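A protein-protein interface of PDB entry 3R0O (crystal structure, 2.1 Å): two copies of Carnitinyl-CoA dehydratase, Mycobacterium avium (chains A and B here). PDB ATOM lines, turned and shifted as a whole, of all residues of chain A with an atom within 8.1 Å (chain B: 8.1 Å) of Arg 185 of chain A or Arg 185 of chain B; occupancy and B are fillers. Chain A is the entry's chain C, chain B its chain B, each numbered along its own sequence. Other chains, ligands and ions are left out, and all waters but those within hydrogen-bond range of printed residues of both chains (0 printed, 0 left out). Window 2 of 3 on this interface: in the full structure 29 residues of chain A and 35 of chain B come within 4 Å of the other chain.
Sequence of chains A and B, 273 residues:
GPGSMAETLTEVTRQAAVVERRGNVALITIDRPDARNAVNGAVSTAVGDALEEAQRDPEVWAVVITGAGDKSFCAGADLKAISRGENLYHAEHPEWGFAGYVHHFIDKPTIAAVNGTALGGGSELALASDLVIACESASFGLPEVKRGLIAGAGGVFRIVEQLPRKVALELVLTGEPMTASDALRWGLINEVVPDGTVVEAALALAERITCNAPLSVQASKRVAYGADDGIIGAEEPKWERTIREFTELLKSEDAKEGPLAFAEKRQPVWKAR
Trp 186 of chain B touches Pro 164 of chain A.
Pro 164 of chain A touches Gly 187 of chain B.
Val 167 of chain A touches Gly 187 of chain B (CG2 to CA, 3.8 Å).
Trp 186 of chain A touches Leu 184 of chain B.
Trp 186 of chain A touches Arg 185 of chain B (CZ3 to O, 3.5 Å).
C of Trp 186 of chain B touches CZ3 of Trp 186 of chain A, at 3.8 Å.
Trp 186 of chain A touches Gly 187 of chain B (CH2 to CA, 3.7 Å).
Of the 17 printed residues of chain B, 4 touch a printed residue of chain A.
Among the printed residues, 8 pairs touch across the chains.
Among the printed residues, no Asp or Glu carboxylate lies within 4 Å of a Lys or Arg side-chain nitrogen of the other chain.
Pro 164 of chain A touches Gly 187 of chain B, but with the chains exchanged Gly 187 of chain A does not touch Pro 164 of chain B (10.3 Å).
Arg 185 of chain A touches its own counterpart, Arg 185 of chain B.
Trp 186 of chain A touches Leu 184 of chain B, but with the chains exchanged Leu 184 of chain A does not touch Trp 186 of chain B (11.4 Å).
Trp 186 of chain A touches Gly 187 of chain B, but with the chains exchanged Gly 187 of chain A does not touch Trp 186 of chain B (9.4 Å).
Positions printed for both chains: 163, 164, 167, 178, 179, 180, 181, 182, 183, 184, 185, 186, 187, 188, 189, 190 and 192.
The backbone carbonyl oxygen (O) of Arg 185 of chain B sits at hydrogen-bond distance from the guanidinium group (NH2) of Arg 185 of chain A (3.0 Å).
Arg 185 of chain B touches just these residues of chain A: Arg 185 (3.0 Å) and Trp 186 (3.5 Å).
Of the printed residues of chain B, Val 167 of chain A touches Gly 187.
Of the printed residues of chain A, Leu 184 of chain B touches Trp 186 (3.8 Å).
Of the printed residues of chain B, Trp 186 of chain A touches Leu 184 (3.8 Å), Arg 185 (3.5 Å), Trp 186 (3.8 Å) and Gly 187 (3.7 Å).
Printed residues of chain A within 4 Å of Trp 186 of chain B: Pro 164 (3.7 Å) and Trp 186 (3.8 Å).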
ATOM      1  N   LEU A 163     -19.505 -12.236  13.729  1.00  0.00           N
ATOM      2  CA  LEU A 163     -20.201 -13.124  14.667  1.00  0.00           C
ATOM      3  C   LEU A 163     -20.261 -12.364  15.976  1.00  0.00           C
ATOM      4  O   LEU A 163     -19.443 -11.441  16.185  1.00  0.00           O
ATOM      5  CB  LEU A 163     -19.416 -14.429  14.901  1.00  0.00           C
ATOM      6  CG  LEU A 163     -19.516 -15.536  13.850  1.00  0.00           C
ATOM      7  CD1 LEU A 163     -18.604 -16.728  14.182  1.00  0.00           C
ATOM      8  CD2 LEU A 163     -20.977 -16.023  13.705  1.00  0.00           C
ATOM      9  N   PRO A 164     -21.193 -12.753  16.888  1.00  0.00           N
ATOM     10  CA  PRO A 164     -21.064 -12.209  18.237  1.00  0.00           C
ATOM     11  C   PRO A 164     -19.691 -12.496  18.797  1.00  0.00           C
ATOM     12  O   PRO A 164     -19.156 -13.608  18.607  1.00  0.00           O
ATOM     13  CB  PRO A 164     -22.100 -13.001  19.032  1.00  0.00           C
ATOM     14  CG  PRO A 164     -23.138 -13.351  18.021  1.00  0.00           C
ATOM     15  CD  PRO A 164     -22.377 -13.621  16.761  1.00  0.00           C
ATOM     16  N   VAL A 167     -18.817 -15.789  20.571  1.00  0.00           N
ATOM     17  CA  VAL A 167     -18.919 -16.887  19.626  1.00  0.00           C
ATOM     18  C   VAL A 167     -17.727 -16.903  18.652  1.00  0.00           C
ATOM     19  O   VAL A 167     -17.190 -17.987  18.354  1.00  0.00           O
ATOM     20  CB  VAL A 167     -20.244 -16.841  18.872  1.00  0.00           C
ATOM     21  CG1 VAL A 167     -20.297 -17.928  17.772  1.00  0.00           C
ATOM     22  CG2 VAL A 167     -21.391 -16.998  19.868  1.00  0.00           C
ATOM     23  N   MET A 178     -17.596 -24.475  12.148  1.00  0.00           N
ATOM     24  CA  MET A 178     -18.967 -24.069  12.344  1.00  0.00           C
ATOM     25  C   MET A 178     -19.713 -24.546  11.108  1.00  0.00           C
ATOM     26  O   MET A 178     -19.248 -24.328   9.980  1.00  0.00           O
ATOM     27  CB  MET A 178     -19.110 -22.542  12.490  1.00  0.00           C
ATOM     28  CG  MET A 178     -20.572 -22.128  12.758  1.00  0.00           C
ATOM     29  SD  MET A 178     -20.781 -20.332  12.879  1.00  0.00           S
ATOM     30  CE  MET A 178     -20.369 -20.091  14.622  1.00  0.00           C
ATOM     31  N   THR A 179     -20.856 -25.189  11.332  1.00  0.00           N
ATOM     32  CA  THR A 179     -21.699 -25.687  10.248  1.00  0.00           C
ATOM     33  C   THR A 179     -22.420 -24.533   9.569  1.00  0.00           C
ATOM     34  O   THR A 179     -22.501 -23.411  10.104  1.00  0.00           O
ATOM     35  CB  THR A 179     -22.766 -26.698  10.764  1.00  0.00           C
ATOM     36  OG1 THR A 179     -23.625 -26.040  11.705  1.00  0.00           O
ATOM     37  CG2 THR A 179     -22.095 -27.868  11.454  1.00  0.00           C
ATOM     38  N   ALA A 180     -22.934 -24.815   8.373  1.00  0.00           N
ATOM     39  CA  ALA A 180     -23.621 -23.812   7.598  1.00  0.00           C
ATOM     40  C   ALA A 180     -24.909 -23.387   8.309  1.00  0.00           C
ATOM     41  O   ALA A 180     -25.233 -22.229   8.295  1.00  0.00           O
ATOM     42  CB  ALA A 180     -23.914 -24.337   6.168  1.00  0.00           C
ATOM     43  N   SER A 181     -25.629 -24.327   8.921  1.00  0.00           N
ATOM     44  CA  SER A 181     -26.876 -24.016   9.631  1.00  0.00           C
ATOM     45  C   SER A 181     -26.642 -23.102  10.835  1.00  0.00           C
ATOM     46  O   SER A 181     -27.415 -22.164  11.054  1.00  0.00           O
ATOM     47  CB  SER A 181     -27.619 -25.298  10.066  1.00  0.00           C
ATOM     48  OG  SER A 181     -26.855 -26.070  11.012  1.00  0.00           O
ATOM     49  N   ASP A 182     -25.603 -23.383  11.622  1.00  0.00           N
ATOM     50  CA  ASP A 182     -25.233 -22.470  12.719  1.00  0.00           C
ATOM     51  C   ASP A 182     -24.803 -21.091  12.221  1.00  0.00           C
ATOM     52  O   ASP A 182     -25.168 -20.086  12.820  1.00  0.00           O
ATOM     53  CB  ASP A 182     -24.129 -23.048  13.596  1.00  0.00           C
ATOM     54  CG  ASP A 182     -24.631 -24.124  14.536  1.00  0.00           C
ATOM     55  OD1 ASP A 182     -25.851 -24.283  14.671  1.00  0.00           O
ATOM     56  OD2 ASP A 182     -23.799 -24.818  15.138  1.00  0.00           O
ATOM     57  N   ALA A 183     -24.018 -21.056  11.145  1.00  0.00           N
ATOM     58  CA  ALA A 183     -23.591 -19.801  10.523  1.00  0.00           C
ATOM     59  C   ALA A 183     -24.794 -18.955  10.105  1.00  0.00           C
ATOM     60  O   ALA A 183     -24.805 -17.739  10.305  1.00  0.00           O
ATOM     61  CB  ALA A 183     -22.707 -20.076   9.312  1.00  0.00           C
ATOM     62  N   LEU A 184     -25.784 -19.628   9.507  1.00  0.00           N
ATOM     63  CA  LEU A 184     -27.040 -19.010   9.109  1.00  0.00           C
ATOM     64  C   LEU A 184     -27.772 -18.431  10.338  1.00  0.00           C
ATOM     65  O   LEU A 184     -28.217 -17.291  10.314  1.00  0.00           O
ATOM     66  CB  LEU A 184     -27.931 -20.032   8.417  1.00  0.00           C
ATOM     67  CG  LEU A 184     -29.215 -19.446   7.849  1.00  0.00           C
ATOM     68  CD1 LEU A 184     -28.911 -18.510   6.647  1.00  0.00           C
ATOM     69  CD2 LEU A 184     -30.210 -20.561   7.466  1.00  0.00           C
ATOM     70  N   ARG A 185     -27.872 -19.233  11.397  1.00  0.00           N
ATOM     71  CA  ARG A 185     -28.546 -18.831  12.645  1.00  0.00           C
ATOM     72  C   ARG A 185     -27.869 -17.590  13.261  1.00  0.00           C
ATOM     73  O   ARG A 185     -28.550 -16.696  13.704  1.00  0.00           O
ATOM     74  CB  ARG A 185     -28.589 -20.021  13.623  1.00  0.00           C
ATOM     75  CG  ARG A 185     -28.986 -19.718  15.076  1.00  0.00           C
ATOM     76  CD  ARG A 185     -27.724 -19.348  15.893  1.00  0.00           C
ATOM     77  NE  ARG A 185     -28.055 -18.872  17.239  1.00  0.00           N
ATOM     78  CZ  ARG A 185     -28.036 -19.633  18.334  1.00  0.00           C
ATOM     79  NH1 ARG A 185     -27.678 -20.918  18.265  1.00  0.00           N
ATOM     80  NH2 ARG A 185     -28.373 -19.098  19.504  1.00  0.00           N
ATOM     81  N   TRP A 186     -26.539 -17.519  13.261  1.00  0.00           N
ATOM     82  CA  TRP A 186     -25.850 -16.326  13.774  1.00  0.00           C
ATOM     83  C   TRP A 186     -25.898 -15.082  12.861  1.00  0.00           C
ATOM     84  O   TRP A 186     -25.619 -13.960  13.305  1.00  0.00           O
ATOM     85  CB  TRP A 186     -24.412 -16.658  14.100  1.00  0.00           C
ATOM     86  CG  TRP A 186     -24.258 -17.617  15.257  1.00  0.00           C
ATOM     87  CD1 TRP A 186     -23.674 -18.850  15.216  1.00  0.00           C
ATOM     88  CD2 TRP A 186     -24.697 -17.426  16.609  1.00  0.00           C
ATOM     89  NE1 TRP A 186     -23.684 -19.425  16.460  1.00  0.00           N
ATOM     90  CE2 TRP A 186     -24.328 -18.586  17.332  1.00  0.00           C
ATOM     91  CE3 TRP A 186     -25.361 -16.391  17.283  1.00  0.00           C
ATOM     92  CZ2 TRP A 186     -24.605 -18.742  18.702  1.00  0.00           C
ATOM     93  CZ3 TRP A 186     -25.648 -16.551  18.650  1.00  0.00           C
ATOM     94  CH2 TRP A 186     -25.251 -17.711  19.343  1.00  0.00           C
ATOM     95  N   GLY A 187     -26.288 -15.264  11.602  1.00  0.00           N
ATOM     96  CA  GLY A 187     -26.207 -14.171  10.619  1.00  0.00           C
ATOM     97  C   GLY A 187     -24.823 -13.998   9.998  1.00  0.00           C
ATOM     98  O   GLY A 187     -24.516 -12.925   9.425  1.00  0.00           O
ATOM     99  N   LEU A 188     -23.972 -15.025  10.126  1.00  0.00           N
ATOM    100  CA  LEU A 188     -22.673 -15.018   9.429  1.00  0.00           C
ATOM    101  C   LEU A 188     -22.840 -15.212   7.907  1.00  0.00           C
ATOM    102  O   LEU A 188     -22.035 -14.734   7.113  1.00  0.00           O
ATOM    103  CB  LEU A 188     -21.728 -16.105  10.008  1.00  0.00           C
ATOM    104  CG  LEU A 188     -20.305 -16.268   9.438  1.00  0.00           C
ATOM    105  CD1 LEU A 188     -19.445 -14.976   9.643  1.00  0.00           C
ATOM    106  CD2 LEU A 188     -19.585 -17.503  10.019  1.00  0.00           C
ATOM    107  N   ILE A 189     -23.864 -15.947   7.508  1.00  0.00           N
ATOM    108  CA  ILE A 189     -24.163 -16.170   6.087  1.00  0.00           C
ATOM    109  C   ILE A 189     -25.623 -15.867   5.819  1.00  0.00           C
ATOM    110  O   ILE A 189     -26.403 -15.676   6.765  1.00  0.00           O
ATOM    111  CB  ILE A 189     -23.777 -17.608   5.631  1.00  0.00           C
ATOM    112  CG1 ILE A 189     -24.642 -18.659   6.358  1.00  0.00           C
ATOM    113  CG2 ILE A 189     -22.260 -17.853   5.912  1.00  0.00           C
ATOM    114  CD1 ILE A 189     -24.525 -20.085   5.750  1.00  0.00           C
ATOM    115  N   ASN A 190     -25.981 -15.794   4.543  1.00  0.00           N
ATOM    116  CA  ASN A 190     -27.284 -15.291   4.171  1.00  0.00           C
ATOM    117  C   ASN A 190     -28.306 -16.359   3.827  1.00  0.00           C
ATOM    118  O   ASN A 190     -29.492 -16.112   3.937  1.00  0.00           O
ATOM    119  CB  ASN A 190     -27.168 -14.285   3.024  1.00  0.00           C
ATOM    120  CG  ASN A 190     -26.280 -13.125   3.383  1.00  0.00           C
ATOM    121  OD1 ASN A 190     -25.073 -13.212   3.210  1.00  0.00           O
ATOM    122  ND2 ASN A 190     -26.866 -12.044   3.931  1.00  0.00           N
ATOM    123  N   VAL A 192     -28.750 -20.986   3.242  1.00  0.00           N
ATOM    124  CA  VAL A 192     -28.245 -22.359   3.150  1.00  0.00           C
ATOM    125  C   VAL A 192     -29.161 -23.105   2.164  1.00  0.00           C
ATOM    126  O   VAL A 192     -30.388 -23.039   2.301  1.00  0.00           O
ATOM    127  CB  VAL A 192     -28.282 -23.114   4.513  1.00  0.00           C
ATOM    128  CG1 VAL A 192     -27.895 -24.633   4.346  1.00  0.00           C
ATOM    129  CG2 VAL A 192     -27.390 -22.435   5.568  1.00  0.00           C
ATOM    130  N   LEU B 163     -23.521  -7.669  22.712  1.00  0.00           N
ATOM    131  CA  LEU B 163     -24.915  -7.987  22.448  1.00  0.00           C
ATOM    132  C   LEU B 163     -25.349  -7.037  21.309  1.00  0.00           C
ATOM    133  O   LEU B 163     -24.706  -5.996  21.090  1.00  0.00           O
ATOM    134  CB  LEU B 163     -25.794  -7.723  23.688  1.00  0.00           C
ATOM    135  CG  LEU B 163     -25.894  -8.716  24.838  1.00  0.00           C
ATOM    136  CD1 LEU B 163     -26.529  -8.049  26.067  1.00  0.00           C
ATOM    137  CD2 LEU B 163     -26.695  -9.980  24.430  1.00  0.00           C
ATOM    138  N   PRO B 164     -26.417  -7.384  20.580  1.00  0.00           N
ATOM    139  CA  PRO B 164     -26.954  -6.422  19.601  1.00  0.00           C
ATOM    140  C   PRO B 164     -27.230  -5.102  20.275  1.00  0.00           C
ATOM    141  O   PRO B 164     -27.720  -5.078  21.409  1.00  0.00           O
ATOM    142  CB  PRO B 164     -28.246  -7.085  19.149  1.00  0.00           C
ATOM    143  CG  PRO B 164     -27.930  -8.602  19.292  1.00  0.00           C
ATOM    144  CD  PRO B 164     -27.143  -8.675  20.553  1.00  0.00           C
ATOM    145  N   VAL B 167     -30.527  -4.391  22.190  1.00  0.00           N
ATOM    146  CA  VAL B 167     -30.638  -5.307  23.333  1.00  0.00           C
ATOM    147  C   VAL B 167     -29.678  -4.886  24.457  1.00  0.00           C
ATOM    148  O   VAL B 167     -30.065  -4.856  25.645  1.00  0.00           O
ATOM    149  CB  VAL B 167     -30.373  -6.771  22.869  1.00  0.00           C
ATOM    150  CG1 VAL B 167     -30.419  -7.770  24.054  1.00  0.00           C
ATOM    151  CG2 VAL B 167     -31.420  -7.169  21.781  1.00  0.00           C
ATOM    152  N   MET B 178     -30.545 -10.396  32.729  1.00  0.00           N
ATOM    153  CA  MET B 178     -30.730 -11.296  31.584  1.00  0.00           C
ATOM    154  C   MET B 178     -30.410 -12.724  32.041  1.00  0.00           C
ATOM    155  O   MET B 178     -29.382 -12.947  32.662  1.00  0.00           O
ATOM    156  CB  MET B 178     -29.788 -10.917  30.418  1.00  0.00           C
ATOM    157  CG  MET B 178     -30.001 -11.756  29.180  1.00  0.00           C
ATOM    158  SD  MET B 178     -28.885 -11.421  27.797  1.00  0.00           S
ATOM    159  CE  MET B 178     -29.685  -9.960  27.099  1.00  0.00           C
ATOM    160  N   THR B 179     -31.269 -13.686  31.717  1.00  0.00           N
ATOM    161  CA  THR B 179     -31.016 -15.062  32.141  1.00  0.00           C
ATOM    162  C   THR B 179     -29.848 -15.681  31.371  1.00  0.00           C
ATOM    163  O   THR B 179     -29.543 -15.244  30.260  1.00  0.00           O
ATOM    164  CB  THR B 179     -32.256 -15.950  31.906  1.00  0.00           C
ATOM    165  OG1 THR B 179     -32.531 -16.005  30.501  1.00  0.00           O
ATOM    166  CG2 THR B 179     -33.492 -15.399  32.696  1.00  0.00           C
ATOM    167  N   ALA B 180     -29.219 -16.703  31.959  1.00  0.00           N
ATOM    168  CA  ALA B 180     -28.177 -17.473  31.281  1.00  0.00           C
ATOM    169  C   ALA B 180     -28.660 -17.959  29.906  1.00  0.00           C
ATOM    170  O   ALA B 180     -27.951 -17.851  28.907  1.00  0.00           O
ATOM    171  CB  ALA B 180     -27.756 -18.661  32.134  1.00  0.00           C
ATOM    172  N   SER B 181     -29.894 -18.451  29.858  1.00  0.00           N
ATOM    173  CA  SER B 181     -30.456 -18.998  28.633  1.00  0.00           C
ATOM    174  C   SER B 181     -30.577 -17.958  27.488  1.00  0.00           C
ATOM    175  O   SER B 181     -30.205 -18.253  26.329  1.00  0.00           O
ATOM    176  CB  SER B 181     -31.777 -19.725  28.940  1.00  0.00           C
ATOM    177  OG  SER B 181     -32.618 -19.749  27.804  1.00  0.00           O
ATOM    178  N   ASP B 182     -31.072 -16.767  27.803  1.00  0.00           N
ATOM    179  CA  ASP B 182     -31.128 -15.677  26.830  1.00  0.00           C
ATOM    180  C   ASP B 182     -29.742 -15.172  26.458  1.00  0.00           C
ATOM    181  O   ASP B 182     -29.523 -14.831  25.300  1.00  0.00           O
ATOM    182  CB  ASP B 182     -31.942 -14.501  27.340  1.00  0.00           C
ATOM    183  CG  ASP B 182     -33.428 -14.728  27.215  1.00  0.00           C
ATOM    184  OD1 ASP B 182     -33.837 -15.621  26.444  1.00  0.00           O
ATOM    185  OD2 ASP B 182     -34.181 -13.995  27.881  1.00  0.00           O
ATOM    186  N   ALA B 183     -28.818 -15.136  27.425  1.00  0.00           N
ATOM    187  CA  ALA B 183     -27.420 -14.772  27.131  1.00  0.00           C
ATOM    188  C   ALA B 183     -26.810 -15.731  26.100  1.00  0.00           C
ATOM    189  O   ALA B 183     -26.059 -15.296  25.232  1.00  0.00           O
ATOM    190  CB  ALA B 183     -26.544 -14.731  28.423  1.00  0.00           C
ATOM    191  N   LEU B 184     -27.146 -17.027  26.198  1.00  0.00           N
ATOM    192  CA  LEU B 184     -26.626 -18.030  25.299  1.00  0.00           C
ATOM    193  C   LEU B 184     -27.215 -17.850  23.896  1.00  0.00           C
ATOM    194  O   LEU B 184     -26.504 -17.895  22.903  1.00  0.00           O
ATOM    195  CB  LEU B 184     -26.962 -19.449  25.809  1.00  0.00           C
ATOM    196  CG  LEU B 184     -26.377 -20.575  24.943  1.00  0.00           C
ATOM    197  CD1 LEU B 184     -24.870 -20.634  25.133  1.00  0.00           C
ATOM    198  CD2 LEU B 184     -27.007 -21.951  25.261  1.00  0.00           C
ATOM    199  N   ARG B 185     -28.524 -17.657  23.841  1.00  0.00           N
ATOM    200  CA  ARG B 185     -29.248 -17.405  22.605  1.00  0.00           C
ATOM    201  C   ARG B 185     -28.687 -16.190  21.814  1.00  0.00           C
ATOM    202  O   ARG B 185     -28.530 -16.269  20.608  1.00  0.00           O
ATOM    203  CB  ARG B 185     -30.750 -17.298  22.934  1.00  0.00           C
ATOM    204  CG  ARG B 185     -31.672 -16.619  21.924  1.00  0.00           C
ATOM    205  CD  ARG B 185     -32.872 -15.964  22.707  1.00  0.00           C
ATOM    206  NE  ARG B 185     -33.730 -15.061  21.914  1.00  0.00           N
ATOM    207  CZ  ARG B 185     -33.372 -14.388  20.818  1.00  0.00           C
ATOM    208  NH1 ARG B 185     -32.136 -14.468  20.335  1.00  0.00           N
ATOM    209  NH2 ARG B 185     -34.266 -13.620  20.199  1.00  0.00           N
ATOM    210  N   TRP B 186     -28.346 -15.107  22.503  1.00  0.00           N
ATOM    211  CA  TRP B 186     -27.734 -13.939  21.875  1.00  0.00           C
ATOM    212  C   TRP B 186     -26.244 -14.113  21.503  1.00  0.00           C
ATOM    213  O   TRP B 186     -25.703 -13.315  20.734  1.00  0.00           O
ATOM    214  CB  TRP B 186     -27.881 -12.712  22.792  1.00  0.00           C
ATOM    215  CG  TRP B 186     -29.314 -12.200  22.894  1.00  0.00           C
ATOM    216  CD1 TRP B 186     -30.057 -12.055  24.036  1.00  0.00           C
ATOM    217  CD2 TRP B 186     -30.160 -11.795  21.806  1.00  0.00           C
ATOM    218  NE1 TRP B 186     -31.325 -11.585  23.720  1.00  0.00           N
ATOM    219  CE2 TRP B 186     -31.405 -11.419  22.358  1.00  0.00           C
ATOM    220  CE3 TRP B 186     -29.979 -11.702  20.410  1.00  0.00           C
ATOM    221  CZ2 TRP B 186     -32.478 -10.954  21.560  1.00  0.00           C
ATOM    222  CZ3 TRP B 186     -31.043 -11.258  19.617  1.00  0.00           C
ATOM    223  CH2 TRP B 186     -32.281 -10.883  20.203  1.00  0.00           C
ATOM    224  N   GLY B 187     -25.576 -15.125  22.065  1.00  0.00           N
ATOM    225  CA  GLY B 187     -24.140 -15.307  21.858  1.00  0.00           C
ATOM    226  C   GLY B 187     -23.287 -14.445  22.779  1.00  0.00           C
ATOM    227  O   GLY B 187     -22.106 -14.242  22.521  1.00  0.00           O
ATOM    228  N   LEU B 188     -23.882 -13.947  23.871  1.00  0.00           N
ATOM    229  CA  LEU B 188     -23.119 -13.265  24.929  1.00  0.00           C
ATOM    230  C   LEU B 188     -22.232 -14.236  25.711  1.00  0.00           C
ATOM    231  O   LEU B 188     -21.173 -13.853  26.198  1.00  0.00           O
ATOM    232  CB  LEU B 188     -24.071 -12.561  25.925  1.00  0.00           C
ATOM    233  CG  LEU B 188     -23.444 -11.730  27.059  1.00  0.00           C
ATOM    234  CD1 LEU B 188     -22.645 -10.545  26.524  1.00  0.00           C
ATOM    235  CD2 LEU B 188     -24.525 -11.259  28.016  1.00  0.00           C
ATOM    236  N   ILE B 189     -22.701 -15.470  25.887  1.00  0.00           N
ATOM    237  CA  ILE B 189     -21.912 -16.489  26.561  1.00  0.00           C
ATOM    238  C   ILE B 189     -21.800 -17.714  25.645  1.00  0.00           C
ATOM    239  O   ILE B 189     -22.488 -17.756  24.607  1.00  0.00           O
ATOM    240  CB  ILE B 189     -22.514 -16.868  27.934  1.00  0.00           C
ATOM    241  CG1 ILE B 189     -23.893 -17.574  27.779  1.00  0.00           C
ATOM    242  CG2 ILE B 189     -22.663 -15.649  28.814  1.00  0.00           C
ATOM    243  CD1 ILE B 189     -24.438 -18.081  29.115  1.00  0.00           C
ATOM    244  N   ASN B 190     -20.958 -18.694  26.009  1.00  0.00           N
ATOM    245  CA  ASN B 190     -20.648 -19.796  25.089  1.00  0.00           C
ATOM    246  C   ASN B 190     -21.389 -21.088  25.374  1.00  0.00           C
ATOM    247  O   ASN B 190     -21.608 -21.874  24.457  1.00  0.00           O
ATOM    248  CB  ASN B 190     -19.152 -20.082  25.020  1.00  0.00           C
ATOM    249  CG  ASN B 190     -18.357 -18.877  24.541  1.00  0.00           C
ATOM    250  OD1 ASN B 190     -18.051 -17.993  25.324  1.00  0.00           O
ATOM    251  ND2 ASN B 190     -18.028 -18.845  23.248  1.00  0.00           N
ATOM    252  N   VAL B 192     -24.282 -23.086  28.489  1.00  0.00           N
ATOM    253  CA  VAL B 192     -25.085 -23.205  29.713  1.00  0.00           C
ATOM    254  C   VAL B 192     -25.061 -24.666  30.171  1.00  0.00           C
ATOM    255  O   VAL B 192     -25.303 -25.594  29.378  1.00  0.00           O
ATOM    256  CB  VAL B 192     -26.540 -22.715  29.531  1.00  0.00           C
ATOM    257  CG1 VAL B 192     -27.398 -22.993  30.776  1.00  0.00           C
ATOM    258  CG2 VAL B 192     -26.563 -21.195  29.249  1.00  0.00           C
